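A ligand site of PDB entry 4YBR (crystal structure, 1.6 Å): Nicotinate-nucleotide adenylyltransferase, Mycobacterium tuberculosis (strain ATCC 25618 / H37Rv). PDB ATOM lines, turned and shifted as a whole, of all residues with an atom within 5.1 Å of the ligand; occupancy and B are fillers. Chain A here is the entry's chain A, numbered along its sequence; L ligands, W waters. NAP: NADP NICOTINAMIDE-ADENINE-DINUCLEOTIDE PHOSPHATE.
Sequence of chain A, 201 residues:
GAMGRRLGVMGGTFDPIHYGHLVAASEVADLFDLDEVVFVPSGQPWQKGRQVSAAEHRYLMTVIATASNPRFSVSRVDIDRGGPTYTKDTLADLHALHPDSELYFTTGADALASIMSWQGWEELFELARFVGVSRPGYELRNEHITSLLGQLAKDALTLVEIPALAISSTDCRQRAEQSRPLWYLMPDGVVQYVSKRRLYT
A ring nitrogen (NE2) of His 18 lies within hydrogen-bond range of the backbone NH of Ser 169 (3.4 Å).
N of His 18 sits at hydrogen-bond distance from ND1 of His 21, 3.2 Å away.
The backbone NH (N) of Thr 87 sits close to the side-chain amide nitrogen (NE2) of Gln 119 (3.2 Å).
O of Gly 12 sits at hydrogen-bond distance from N of Ser 42, at 2.9 Å.
The backbone NH (N) of Val 133 is in hydrogen-bond range of the backbone carbonyl oxygen (O) of Thr 107.
The side-chain hydroxyl of Thr 107 is in hydrogen-bond range of the backbone carbonyl oxygen of Gly 11, at 2.7 Å.
OG of Ser 42 sits at hydrogen-bond distance from OG1 of Thr 85 (3.2 Å).
N of Ala 109 sits at hydrogen-bond distance from O of Val 133 (2.9 Å).
A nitrogen (N7N) of the ligand lies close to the indole nitrogen (NE1) of Trp 118 (3.3 Å).
Phe 14 touches the ligand (CE1 to N6A, 3.9 Å).
CG2 of Thr 85 touches O2D of the ligand, at 3.4 Å.
Phe 105 touches the ligand.
Thr 106 touches the ligand.
Gly 108 touches the ligand (CA to O4B, 3.2 Å).
Ala 111 touches the ligand (CB to C5D, 3.6 Å).
Ile 115 touches the ligand.
Val 133 touches the ligand (CG2 to C2A, 3.2 Å).
Leu 165 touches the ligand (CD2 to C2A, 3.96 Å).
CA of Ser 168 touches O1X of the ligand, 3.4 Å away.
Water W3 lies within hydrogen-bond range of an oxygen (O2X) of the ligand (2.6 Å), the backbone NH (N) of Phe 14 (3.3 Å) and the side-chain hydroxyl (OG1) of Thr 13 (3.3 Å).
Water W10 lies within hydrogen-bond range of an oxygen (O3X) of the ligand, the side-chain hydroxyl of Thr 170 and the backbone NH of Ser 169.
Water W6 lies within hydrogen-bond range of OD2 of Asp 78 (2.6 Å), O3D of the ligand (2.7 Å) and O of Val 40 (2.8 Å).
Water W9 lies within hydrogen-bond range of an oxygen (O2A) of the ligand (2.7 Å) and the side-chain hydroxyl of Thr 13 (3.3 Å).
Water W5 lies within hydrogen-bond range of an oxygen (O1X) of the ligand (2.7 Å), the backbone carbonyl oxygen (O) of Ile 167 (2.9 Å) and the backbone carbonyl oxygen (O) of Leu 165 (3.3 Å).
Water W4 bridges O3B of the ligand (3.0 Å) and O of Val 133 (3.5 Å).
The side-chain hydroxyl of Thr 107 lies close to a nitrogen (N7A) of the ligand, at 3.2 Å.
N of Thr 87 lies within hydrogen-bond range of O7N of the ligand (3.2 Å).
The side-chain sulfur (SD) of Met 10 sits close to a nitrogen (N6A) of the ligand (3.6 Å).
The side-chain amide nitrogen (NE2) of Gln 119 sits at hydrogen-bond distance from an oxygen (O7N) of the ligand, at 2.5 Å.
The backbone NH (N) of Thr 13 is in hydrogen-bond range of an oxygen (O1N) of the ligand, 3.0 Å away.
OG of Ser 169 is in hydrogen-bond range of O1X of the ligand (3.5 Å).
N of Ser 169 lies within hydrogen-bond range of O1X of the ligand (2.9 Å).
The backbone NH (N) of Gly 12 sits at hydrogen-bond distance from an oxygen (O3D) of the ligand (3.3 Å).
The side-chain hydroxyl of Ser 42 is in hydrogen-bond range of an oxygen (O2D) of the ligand, at 2.8 Å.
The side-chain hydroxyl of Thr 87 is in hydrogen-bond range of an oxygen (O7N) of the ligand, 3.2 Å away.
A ring nitrogen (NE2) of His 21 sits at hydrogen-bond distance from an oxygen (O2X) of the ligand (2.6 Å).
The backbone carbonyl oxygen of Gly 11 is in hydrogen-bond range of a nitrogen (N6A) of the ligand (2.9 Å).
NE2 of His 18 is in hydrogen-bond range of O1X of the ligand, 2.8 Å away.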
ATOM      1  N   MET A  10      15.682  21.254  -7.269  1.00  0.00           N
ATOM      2  CA  MET A  10      14.226  21.151  -7.305  1.00  0.00           C
ATOM      3  C   MET A  10      13.692  22.444  -7.850  1.00  0.00           C
ATOM      4  O   MET A  10      13.628  23.445  -7.146  1.00  0.00           O
ATOM      5  CB  MET A  10      13.651  20.917  -5.906  1.00  0.00           C
ATOM      6  CG  MET A  10      13.556  19.477  -5.446  1.00  0.00           C
ATOM      7  SD  MET A  10      12.053  18.655  -6.042  1.00  0.00           S
ATOM      8  CE  MET A  10      10.781  19.427  -5.059  1.00  0.00           C
ATOM      9  N   GLY A  11      13.316  22.429  -9.126  1.00  0.00           N
ATOM     10  CA  GLY A  11      12.796  23.608  -9.778  1.00  0.00           C
ATOM     11  C   GLY A  11      11.270  23.562  -9.772  1.00  0.00           C
ATOM     12  O   GLY A  11      10.695  22.526 -10.062  1.00  0.00           O
ATOM     13  N   GLY A  12      10.654  24.683  -9.436  1.00  0.00           N
ATOM     14  CA  GLY A  12       9.198  24.799  -9.358  1.00  0.00           C
ATOM     15  C   GLY A  12       8.776  26.207  -9.052  1.00  0.00           C
ATOM     16  O   GLY A  12       9.585  27.030  -8.601  1.00  0.00           O
ATOM     17  N   THR A  13       7.503  26.526  -9.271  1.00  0.00           N
ATOM     18  CA  THR A  13       6.986  27.837  -8.845  1.00  0.00           C
ATOM     19  C   THR A  13       6.736  27.869  -7.354  1.00  0.00           C
ATOM     20  O   THR A  13       6.896  28.918  -6.754  1.00  0.00           O
ATOM     21  CB  THR A  13       5.704  28.312  -9.566  1.00  0.00           C
ATOM     22  OG1 THR A  13       4.680  27.323  -9.414  1.00  0.00           O
ATOM     23  CG2 THR A  13       6.012  28.603 -11.038  1.00  0.00           C
ATOM     24  N   PHE A  14       6.343  26.735  -6.761  1.00  0.00           N
ATOM     25  CA  PHE A  14       6.118  26.608  -5.310  1.00  0.00           C
ATOM     26  C   PHE A  14       5.127  27.673  -4.785  1.00  0.00           C
ATOM     27  O   PHE A  14       5.460  28.529  -3.958  1.00  0.00           O
ATOM     28  CB  PHE A  14       7.460  26.639  -4.536  1.00  0.00           C
ATOM     29  CG  PHE A  14       8.463  25.612  -5.007  1.00  0.00           C
ATOM     30  CD1 PHE A  14       8.139  24.256  -5.044  1.00  0.00           C
ATOM     31  CD2 PHE A  14       9.723  25.991  -5.409  1.00  0.00           C
ATOM     32  CE1 PHE A  14       9.050  23.306  -5.493  1.00  0.00           C
ATOM     33  CE2 PHE A  14      10.656  25.051  -5.853  1.00  0.00           C
ATOM     34  CZ  PHE A  14      10.327  23.707  -5.892  1.00  0.00           C
ATOM     35  N   HIS A  18       4.435  22.493  -0.601  1.00  0.00           N
ATOM     36  CA  HIS A  18       3.600  21.612   0.209  1.00  0.00           C
ATOM     37  C   HIS A  18       4.350  20.301   0.442  1.00  0.00           C
ATOM     38  O   HIS A  18       5.446  20.093  -0.083  1.00  0.00           O
ATOM     39  CB  HIS A  18       2.197  21.402  -0.417  1.00  0.00           C
ATOM     40  CG  HIS A  18       2.227  20.916  -1.817  1.00  0.00           C
ATOM     41  ND1 HIS A  18       2.738  19.688  -2.156  1.00  0.00           N
ATOM     42  CD2 HIS A  18       1.816  21.491  -2.977  1.00  0.00           C
ATOM     43  CE1 HIS A  18       2.669  19.519  -3.465  1.00  0.00           C
ATOM     44  NE2 HIS A  18       2.112  20.602  -3.987  1.00  0.00           N
ATOM     45  N   HIS A  21       5.889  18.248  -2.499  1.00  0.00           N
ATOM     46  CA  HIS A  21       7.231  18.669  -2.960  1.00  0.00           C
ATOM     47  C   HIS A  21       8.322  18.163  -2.031  1.00  0.00           C
ATOM     48  O   HIS A  21       9.383  17.728  -2.475  1.00  0.00           O
ATOM     49  CB  HIS A  21       7.344  20.184  -3.007  1.00  0.00           C
ATOM     50  CG  HIS A  21       6.378  20.828  -3.937  1.00  0.00           C
ATOM     51  ND1 HIS A  21       5.442  21.735  -3.504  1.00  0.00           N
ATOM     52  CD2 HIS A  21       6.198  20.705  -5.275  1.00  0.00           C
ATOM     53  CE1 HIS A  21       4.746  22.182  -4.540  1.00  0.00           C
ATOM     54  NE2 HIS A  21       5.178  21.566  -5.625  1.00  0.00           N
ATOM     55  N   ALA A  24       8.725  14.450  -2.450  1.00  0.00           N
ATOM     56  CA  ALA A  24       9.415  14.239  -3.755  1.00  0.00           C
ATOM     57  C   ALA A  24      10.919  14.483  -3.634  1.00  0.00           C
ATOM     58  O   ALA A  24      11.728  13.658  -4.073  1.00  0.00           O
ATOM     59  CB  ALA A  24       8.818  15.120  -4.831  1.00  0.00           C
ATOM     60  N   VAL A  40      14.737  25.759  -5.966  1.00  0.00           N
ATOM     61  CA  VAL A  40      14.909  26.967  -6.759  1.00  0.00           C
ATOM     62  C   VAL A  40      13.530  27.438  -7.224  1.00  0.00           C
ATOM     63  O   VAL A  40      13.025  26.941  -8.249  1.00  0.00           O
ATOM     64  CB  VAL A  40      15.839  26.754  -7.968  1.00  0.00           C
ATOM     65  CG1 VAL A  40      16.102  28.092  -8.649  1.00  0.00           C
ATOM     66  CG2 VAL A  40      17.137  26.080  -7.532  1.00  0.00           C
ATOM     67  N   SER A  42      10.992  29.453  -9.235  1.00  0.00           N
ATOM     68  CA  SER A  42      11.130  29.941 -10.585  1.00  0.00           C
ATOM     69  C   SER A  42      10.738  31.400 -10.641  1.00  0.00           C
ATOM     70  O   SER A  42      10.084  31.930  -9.707  1.00  0.00           O
ATOM     71  CB  SER A  42      10.267  29.110 -11.549  1.00  0.00           C
ATOM     72  OG  SER A  42      10.631  29.339 -12.886  1.00  0.00           O
ATOM     73  N   ASP A  78      17.045  31.942  -9.827  1.00  0.00           N
ATOM     74  CA  ASP A  78      15.998  32.244 -10.829  1.00  0.00           C
ATOM     75  C   ASP A  78      15.201  33.521 -10.532  1.00  0.00           C
ATOM     76  O   ASP A  78      14.855  34.276 -11.461  1.00  0.00           O
ATOM     77  CB  ASP A  78      15.017  31.075 -10.992  1.00  0.00           C
ATOM     78  CG  ASP A  78      15.643  29.867 -11.691  1.00  0.00           C
ATOM     79  OD1 ASP A  78      16.703  29.992 -12.332  1.00  0.00           O
ATOM     80  OD2 ASP A  78      15.025  28.773 -11.633  1.00  0.00           O
ATOM     81  N   THR A  85      12.341  32.263 -16.737  1.00  0.00           N
ATOM     82  CA  THR A  85      13.286  31.277 -16.295  1.00  0.00           C
ATOM     83  C   THR A  85      13.550  30.229 -17.354  1.00  0.00           C
ATOM     84  O   THR A  85      12.651  29.517 -17.773  1.00  0.00           O
ATOM     85  CB  THR A  85      12.779  30.626 -15.011  1.00  0.00           C
ATOM     86  OG1 THR A  85      12.569  31.661 -14.043  1.00  0.00           O
ATOM     87  CG2 THR A  85      13.786  29.620 -14.514  1.00  0.00           C
ATOM     88  N   TYR A  86      14.819  30.156 -17.740  1.00  0.00           N
ATOM     89  CA  TYR A  86      15.330  29.157 -18.651  1.00  0.00           C
ATOM     90  C   TYR A  86      16.173  28.232 -17.804  1.00  0.00           C
ATOM     91  O   TYR A  86      17.083  28.696 -17.139  1.00  0.00           O
ATOM     92  CB  TYR A  86      16.180  29.811 -19.732  1.00  0.00           C
ATOM     93  CG  TYR A  86      15.426  30.843 -20.551  1.00  0.00           C
ATOM     94  CD1 TYR A  86      14.123  30.595 -21.007  1.00  0.00           C
ATOM     95  CD2 TYR A  86      16.006  32.071 -20.847  1.00  0.00           C
ATOM     96  CE1 TYR A  86      13.430  31.550 -21.743  1.00  0.00           C
ATOM     97  CE2 TYR A  86      15.318  33.024 -21.599  1.00  0.00           C
ATOM     98  CZ  TYR A  86      14.038  32.748 -22.046  1.00  0.00           C
ATOM     99  OH  TYR A  86      13.322  33.666 -22.773  1.00  0.00           O
ATOM    100  N   THR A  87      15.824  26.955 -17.819  1.00  0.00           N
ATOM    101  CA  THR A  87      16.543  25.914 -17.062  1.00  0.00           C
ATOM    102  C   THR A  87      18.052  25.851 -17.371  1.00  0.00           C
ATOM    103  O   THR A  87      18.844  25.599 -16.462  1.00  0.00           O
ATOM    104  CB  THR A  87      15.829  24.562 -17.214  1.00  0.00           C
ATOM    105  OG1 THR A  87      14.523  24.665 -16.637  1.00  0.00           O
ATOM    106  CG2 THR A  87      16.546  23.432 -16.524  1.00  0.00           C
ATOM    107  N   PHE A 105      18.513  17.691 -11.919  1.00  0.00           N
ATOM    108  CA  PHE A 105      17.414  18.653 -12.023  1.00  0.00           C
ATOM    109  C   PHE A 105      16.098  17.907 -11.918  1.00  0.00           C
ATOM    110  O   PHE A 105      15.825  17.010 -12.719  1.00  0.00           O
ATOM    111  CB  PHE A 105      17.453  19.470 -13.301  1.00  0.00           C
ATOM    112  CG  PHE A 105      16.425  20.556 -13.329  1.00  0.00           C
ATOM    113  CD1 PHE A 105      16.671  21.781 -12.731  1.00  0.00           C
ATOM    114  CD2 PHE A 105      15.170  20.341 -13.907  1.00  0.00           C
ATOM    115  CE1 PHE A 105      15.715  22.778 -12.720  1.00  0.00           C
ATOM    116  CE2 PHE A 105      14.214  21.350 -13.914  1.00  0.00           C
ATOM    117  CZ  PHE A 105      14.476  22.580 -13.319  1.00  0.00           C
ATOM    118  N   THR A 106      15.286  18.331 -10.959  1.00  0.00           N
ATOM    119  CA  THR A 106      14.074  17.630 -10.576  1.00  0.00           C
ATOM    120  C   THR A 106      12.877  18.570 -10.687  1.00  0.00           C
ATOM    121  O   THR A 106      12.863  19.675 -10.098  1.00  0.00           O
ATOM    122  CB  THR A 106      14.175  17.070  -9.137  1.00  0.00           C
ATOM    123  OG1 THR A 106      15.332  16.220  -8.996  1.00  0.00           O
ATOM    124  CG2 THR A 106      12.950  16.249  -8.796  1.00  0.00           C
ATOM    125  N   THR A 107      11.842  18.148 -11.409  1.00  0.00           N
ATOM    126  CA  THR A 107      10.612  18.918 -11.467  1.00  0.00           C
ATOM    127  C   THR A 107       9.475  18.003 -11.888  1.00  0.00           C
ATOM    128  O   THR A 107       9.691  16.807 -12.088  1.00  0.00           O
ATOM    129  CB  THR A 107      10.738  20.161 -12.390  1.00  0.00           C
ATOM    130  OG1 THR A 107       9.654  21.043 -12.128  1.00  0.00           O
ATOM    131  CG2 THR A 107      10.794  19.795 -13.895  1.00  0.00           C
ATOM    132  N   GLY A 108       8.284  18.558 -11.983  1.00  0.00           N
ATOM    133  CA  GLY A 108       7.118  17.776 -12.416  1.00  0.00           C
ATOM    134  C   GLY A 108       7.311  17.281 -13.818  1.00  0.00           C
ATOM    135  O   GLY A 108       7.908  17.972 -14.648  1.00  0.00           O
ATOM    136  N   ALA A 109       6.829  16.069 -14.086  1.00  0.00           N
ATOM    137  CA  ALA A 109       7.010  15.438 -15.414  1.00  0.00           C
ATOM    138  C   ALA A 109       6.438  16.280 -16.545  1.00  0.00           C
ATOM    139  O   ALA A 109       7.097  16.411 -17.593  1.00  0.00           O
ATOM    140  CB  ALA A 109       6.423  14.038 -15.412  1.00  0.00           C
ATOM    141  N   ASP A 110       5.266  16.897 -16.346  1.00  0.00           N
ATOM    142  CA  ASP A 110       4.697  17.851 -17.329  1.00  0.00           C
ATOM    143  C   ASP A 110       5.624  19.022 -17.668  1.00  0.00           C
ATOM    144  O   ASP A 110       5.772  19.404 -18.825  1.00  0.00           O
ATOM    145  CB  ASP A 110       3.359  18.444 -16.849  1.00  0.00           C
ATOM    146  CG  ASP A 110       2.154  17.534 -17.109  1.00  0.00           C
ATOM    147  OD1 ASP A 110       2.208  16.643 -17.981  1.00  0.00           O
ATOM    148  OD2 ASP A 110       1.131  17.745 -16.425  1.00  0.00           O
ATOM    149  N   ALA A 111       6.251  19.607 -16.659  1.00  0.00           N
ATOM    150  CA  ALA A 111       7.180  20.724 -16.878  1.00  0.00           C
ATOM    151  C   ALA A 111       8.433  20.276 -17.604  1.00  0.00           C
ATOM    152  O   ALA A 111       8.982  21.021 -18.422  1.00  0.00           O
ATOM    153  CB  ALA A 111       7.543  21.375 -15.569  1.00  0.00           C
ATOM    154  N   SER A 114       7.935  20.287 -21.261  1.00  0.00           N
ATOM    155  CA  SER A 114       8.069  21.630 -21.829  1.00  0.00           C
ATOM    156  C   SER A 114       9.525  22.071 -21.954  1.00  0.00           C
ATOM    157  O   SER A 114       9.922  22.587 -23.004  1.00  0.00           O
ATOM    158  CB  SER A 114       7.262  22.653 -21.063  1.00  0.00           C
ATOM    159  OG  SER A 114       5.897  22.402 -21.332  1.00  0.00           O
ATOM    160  N   ILE A 115      10.316  21.853 -20.897  1.00  0.00           N
ATOM    161  CA  ILE A 115      11.732  22.230 -20.920  1.00  0.00           C
ATOM    162  C   ILE A 115      12.432  21.611 -22.134  1.00  0.00           C
ATOM    163  O   ILE A 115      13.055  22.312 -22.921  1.00  0.00           O
ATOM    164  CB  ILE A 115      12.466  21.811 -19.640  1.00  0.00           C
ATOM    165  CG1 ILE A 115      11.980  22.643 -18.438  1.00  0.00           C
ATOM    166  CG2 ILE A 115      13.972  21.979 -19.770  1.00  0.00           C
ATOM    167  CD1 ILE A 115      12.138  21.945 -17.115  1.00  0.00           C
ATOM    168  N   TRP A 118      11.827  22.827 -26.210  1.00  0.00           N
ATOM    169  CA  TRP A 118      12.398  24.005 -26.883  1.00  0.00           C
ATOM    170  C   TRP A 118      13.671  24.619 -26.291  1.00  0.00           C
ATOM    171  O   TRP A 118      14.338  25.382 -26.993  1.00  0.00           O
ATOM    172  CB  TRP A 118      11.309  25.083 -27.036  1.00  0.00           C
ATOM    173  CG  TRP A 118      11.028  25.830 -25.793  1.00  0.00           C
ATOM    174  CD1 TRP A 118      10.097  25.528 -24.843  1.00  0.00           C
ATOM    175  CD2 TRP A 118      11.682  27.018 -25.338  1.00  0.00           C
ATOM    176  NE1 TRP A 118      10.138  26.442 -23.826  1.00  0.00           N
ATOM    177  CE2 TRP A 118      11.104  27.377 -24.110  1.00  0.00           C
ATOM    178  CE3 TRP A 118      12.725  27.807 -25.859  1.00  0.00           C
ATOM    179  CZ2 TRP A 118      11.523  28.497 -23.395  1.00  0.00           C
ATOM    180  CZ3 TRP A 118      13.136  28.915 -25.146  1.00  0.00           C
ATOM    181  CH2 TRP A 118      12.544  29.251 -23.938  1.00  0.00           C
ATOM    182  N   GLN A 119      14.017  24.281 -25.043  1.00  0.00           N
ATOM    183  CA  GLN A 119      15.168  24.894 -24.340  1.00  0.00           C
ATOM    184  C   GLN A 119      16.539  24.584 -24.967  1.00  0.00           C
ATOM    185  O   GLN A 119      17.463  25.389 -24.843  1.00  0.00           O
ATOM    186  CB  GLN A 119      15.153  24.437 -22.858  1.00  0.00           C
ATOM    187  CG  GLN A 119      16.297  24.845 -21.930  1.00  0.00           C
ATOM    188  CD  GLN A 119      16.200  26.252 -21.365  1.00  0.00           C
ATOM    189  OE1 GLN A 119      17.200  26.960 -21.296  1.00  0.00           O
ATOM    190  NE2 GLN A 119      15.027  26.639 -20.918  1.00  0.00           N
ATOM    191  N   VAL A 133       8.996  14.061 -11.716  1.00  0.00           N
ATOM    192  CA  VAL A 133       8.197  13.469 -10.650  1.00  0.00           C
ATOM    193  C   VAL A 133       6.751  13.709 -10.952  1.00  0.00           C
ATOM    194  O   VAL A 133       6.397  14.736 -11.515  1.00  0.00           O
ATOM    195  CB  VAL A 133       8.534  14.000  -9.236  1.00  0.00           C
ATOM    196  CG1 VAL A 133       9.904  13.487  -8.812  1.00  0.00           C
ATOM    197  CG2 VAL A 133       8.444  15.503  -9.158  1.00  0.00           C
ATOM    198  N   LEU A 165       2.335  13.310  -4.182  1.00  0.00           N
ATOM    199  CA  LEU A 165       2.021  14.339  -5.185  1.00  0.00           C
ATOM    200  C   LEU A 165       0.549  14.380  -5.604  1.00  0.00           C
ATOM    201  O   LEU A 165       0.145  15.219  -6.418  1.00  0.00           O
ATOM    202  CB  LEU A 165       2.965  14.249  -6.381  1.00  0.00           C
ATOM    203  CG  LEU A 165       4.411  14.703  -6.083  1.00  0.00           C
ATOM    204  CD1 LEU A 165       5.384  14.387  -7.235  1.00  0.00           C
ATOM    205  CD2 LEU A 165       4.444  16.193  -5.741  1.00  0.00           C
ATOM    206  N   ILE A 167      -1.226  15.624  -3.466  1.00  0.00           N
ATOM    207  CA  ILE A 167      -1.305  16.986  -2.935  1.00  0.00           C
ATOM    208  C   ILE A 167      -0.772  17.922  -4.007  1.00  0.00           C
ATOM    209  O   ILE A 167       0.343  17.729  -4.486  1.00  0.00           O
ATOM    210  CB  ILE A 167      -0.464  17.138  -1.631  1.00  0.00           C
ATOM    211  CG1 ILE A 167      -0.963  16.164  -0.540  1.00  0.00           C
ATOM    212  CG2 ILE A 167      -0.531  18.572  -1.102  1.00  0.00           C
ATOM    213  CD1 ILE A 167      -0.042  16.093   0.684  1.00  0.00           C
ATOM    214  N   SER A 168      -1.577  18.903  -4.421  1.00  0.00           N
ATOM    215  CA  SER A 168      -1.152  19.832  -5.487  1.00  0.00           C
ATOM    216  C   SER A 168      -1.265  21.269  -4.977  1.00  0.00           C
ATOM    217  O   SER A 168      -2.092  21.575  -4.126  1.00  0.00           O
ATOM    218  CB  SER A 168      -1.985  19.651  -6.756  1.00  0.00           C
ATOM    219  OG  SER A 168      -3.258  20.210  -6.544  1.00  0.00           O
ATOM    220  N   SER A 169      -0.456  22.147  -5.547  1.00  0.00           N
ATOM    221  CA  SER A 169      -0.523  23.570  -5.203  1.00  0.00           C
ATOM    222  C   SER A 169      -1.859  24.164  -5.625  1.00  0.00           C
ATOM    223  O   SER A 169      -2.401  25.021  -4.963  1.00  0.00           O
ATOM    224  CB  SER A 169       0.607  24.344  -5.855  1.00  0.00           C
ATOM    225  OG  SER A 169       1.859  23.932  -5.358  1.00  0.00           O
ATOM    226  N   THR A 170      -2.405  23.666  -6.739  1.00  0.00           N
ATOM    227  CA  THR A 170      -3.716  24.144  -7.180  1.00  0.00           C
ATOM    228  C   THR A 170      -4.771  23.861  -6.127  1.00  0.00           C
ATOM    229  O   THR A 170      -5.556  24.744  -5.789  1.00  0.00           O
ATOM    230  CB  THR A 170      -4.112  23.505  -8.524  1.00  0.00           C
ATOM    231  OG1 THR A 170      -3.115  23.858  -9.496  1.00  0.00           O
ATOM    232  CG2 THR A 170      -5.463  24.042  -8.975  1.00  0.00           C
HETATM  233  PA  NAP L   1       3.917  23.716 -13.467  1.00  0.00           P
HETATM  234  O1A NAP L   1       3.359  23.822 -14.846  1.00  0.00           O
HETATM  235  O2A NAP L   1       3.250  24.681 -12.471  1.00  0.00           O
HETATM  236  O5B NAP L   1       3.891  22.196 -12.872  1.00  0.00           O
HETATM  237  C5B NAP L   1       3.575  21.056 -13.701  1.00  0.00           C
HETATM  238  C4B NAP L   1       3.365  19.911 -12.744  1.00  0.00           C
HETATM  239  O4B NAP L   1       4.604  19.661 -12.041  1.00  0.00           O
HETATM  240  C3B NAP L   1       2.319  20.149 -11.660  1.00  0.00           C
HETATM  241  O3B NAP L   1       1.688  18.913 -11.348  1.00  0.00           O
HETATM  242  C2B NAP L   1       3.158  20.608 -10.473  1.00  0.00           C
HETATM  243  O2B NAP L   1       2.528  20.361  -9.202  1.00  0.00           O
HETATM  244  C1B NAP L   1       4.412  19.759 -10.642  1.00  0.00           C
HETATM  245  N9A NAP L   1       5.653  20.282 -10.063  1.00  0.00           N
HETATM  246  C8A NAP L   1       6.336  21.404 -10.430  1.00  0.00           C
HETATM  247  N7A NAP L   1       7.506  21.542  -9.857  1.00  0.00           N
HETATM  248  C5A NAP L   1       7.602  20.420  -9.046  1.00  0.00           C
HETATM  249  C6A NAP L   1       8.632  19.923  -8.236  1.00  0.00           C
HETATM  250  N6A NAP L   1       9.839  20.508  -8.124  1.00  0.00           N
HETATM  251  N1A NAP L   1       8.418  18.750  -7.590  1.00  0.00           N
HETATM  252  C2A NAP L   1       7.247  18.127  -7.768  1.00  0.00           C
HETATM  253  N3A NAP L   1       6.210  18.487  -8.520  1.00  0.00           N
HETATM  254  C4A NAP L   1       6.445  19.642  -9.146  1.00  0.00           C
HETATM  255  O3  NAP L   1       5.490  23.961 -13.482  1.00  0.00           O
HETATM  256  PN  NAP L   1       6.384  24.980 -12.633  1.00  0.00           P
HETATM  257  O1N NAP L   1       6.284  24.631 -11.189  1.00  0.00           O
HETATM  258  O2N NAP L   1       5.965  26.325 -13.091  1.00  0.00           O
HETATM  259  O5D NAP L   1       7.843  24.744 -13.242  1.00  0.00           O
HETATM  260  C5D NAP L   1       8.651  23.593 -12.927  1.00  0.00           C
HETATM  261  C4D NAP L   1      10.108  23.852 -13.252  1.00  0.00           C
HETATM  262  O4D NAP L   1      10.304  23.765 -14.687  1.00  0.00           O
HETATM  263  C3D NAP L   1      10.681  25.197 -12.820  1.00  0.00           C
HETATM  264  O3D NAP L   1      12.044  25.078 -12.401  1.00  0.00           O
HETATM  265  C2D NAP L   1      10.618  26.021 -14.103  1.00  0.00           C
HETATM  266  O2D NAP L   1      11.616  27.023 -14.132  1.00  0.00           O
HETATM  267  C1D NAP L   1      10.922  24.939 -15.137  1.00  0.00           C
HETATM  268  N1N NAP L   1      10.407  25.274 -16.522  1.00  0.00           N
HETATM  269  C2N NAP L   1      11.350  25.597 -17.423  1.00  0.00           C
HETATM  270  C3N NAP L   1      11.002  25.899 -18.736  1.00  0.00           C
HETATM  271  C7N NAP L   1      12.107  26.030 -19.756  1.00  0.00           C
HETATM  272  O7N NAP L   1      13.283  25.780 -19.426  1.00  0.00           O
HETATM  273  N7N NAP L   1      11.796  26.358 -21.000  1.00  0.00           N
HETATM  274  C4N NAP L   1       9.645  25.904 -19.078  1.00  0.00           C
HETATM  275  C5N NAP L   1       8.693  25.572 -18.125  1.00  0.00           C
HETATM  276  C6N NAP L   1       9.092  25.252 -16.845  1.00  0.00           C
HETATM  277  P2B NAP L   1       2.474  21.522  -8.064  1.00  0.00           P
HETATM  278  O1X NAP L   1       1.823  20.799  -6.808  1.00  0.00           O
HETATM  279  O2X NAP L   1       3.890  22.044  -7.882  1.00  0.00           O
HETATM  280  O3X NAP L   1       1.538  22.672  -8.631  1.00  0.00           O
HETATM  281  O   HOH W   1       1.380  23.888 -10.869  1.00  0.00           O
HETATM  282  O   HOH W   2      -0.063  18.455  -9.373  1.00  0.00           O
HETATM  283  O   HOH W   3       5.196  24.210  -8.505  1.00  0.00           O
HETATM  284  O   HOH W   4       3.367  16.388 -11.300  1.00  0.00           O
HETATM  285  O   HOH W   5       1.483  18.097  -7.146  1.00  0.00           O
HETATM  286  O   HOH W   6      13.055  27.117 -11.027  1.00  0.00           O
HETATM  287  O   HOH W   7      14.787  26.041 -14.027  1.00  0.00           O
HETATM  288  O   HOH W   8       3.696  16.890  -8.749  1.00  0.00           O
HETATM  289  O   HOH W   9       3.040  27.332 -12.312  1.00  0.00           O
HETATM  290  O   HOH W  10      -1.016  22.223  -8.980  1.00  0.00           O
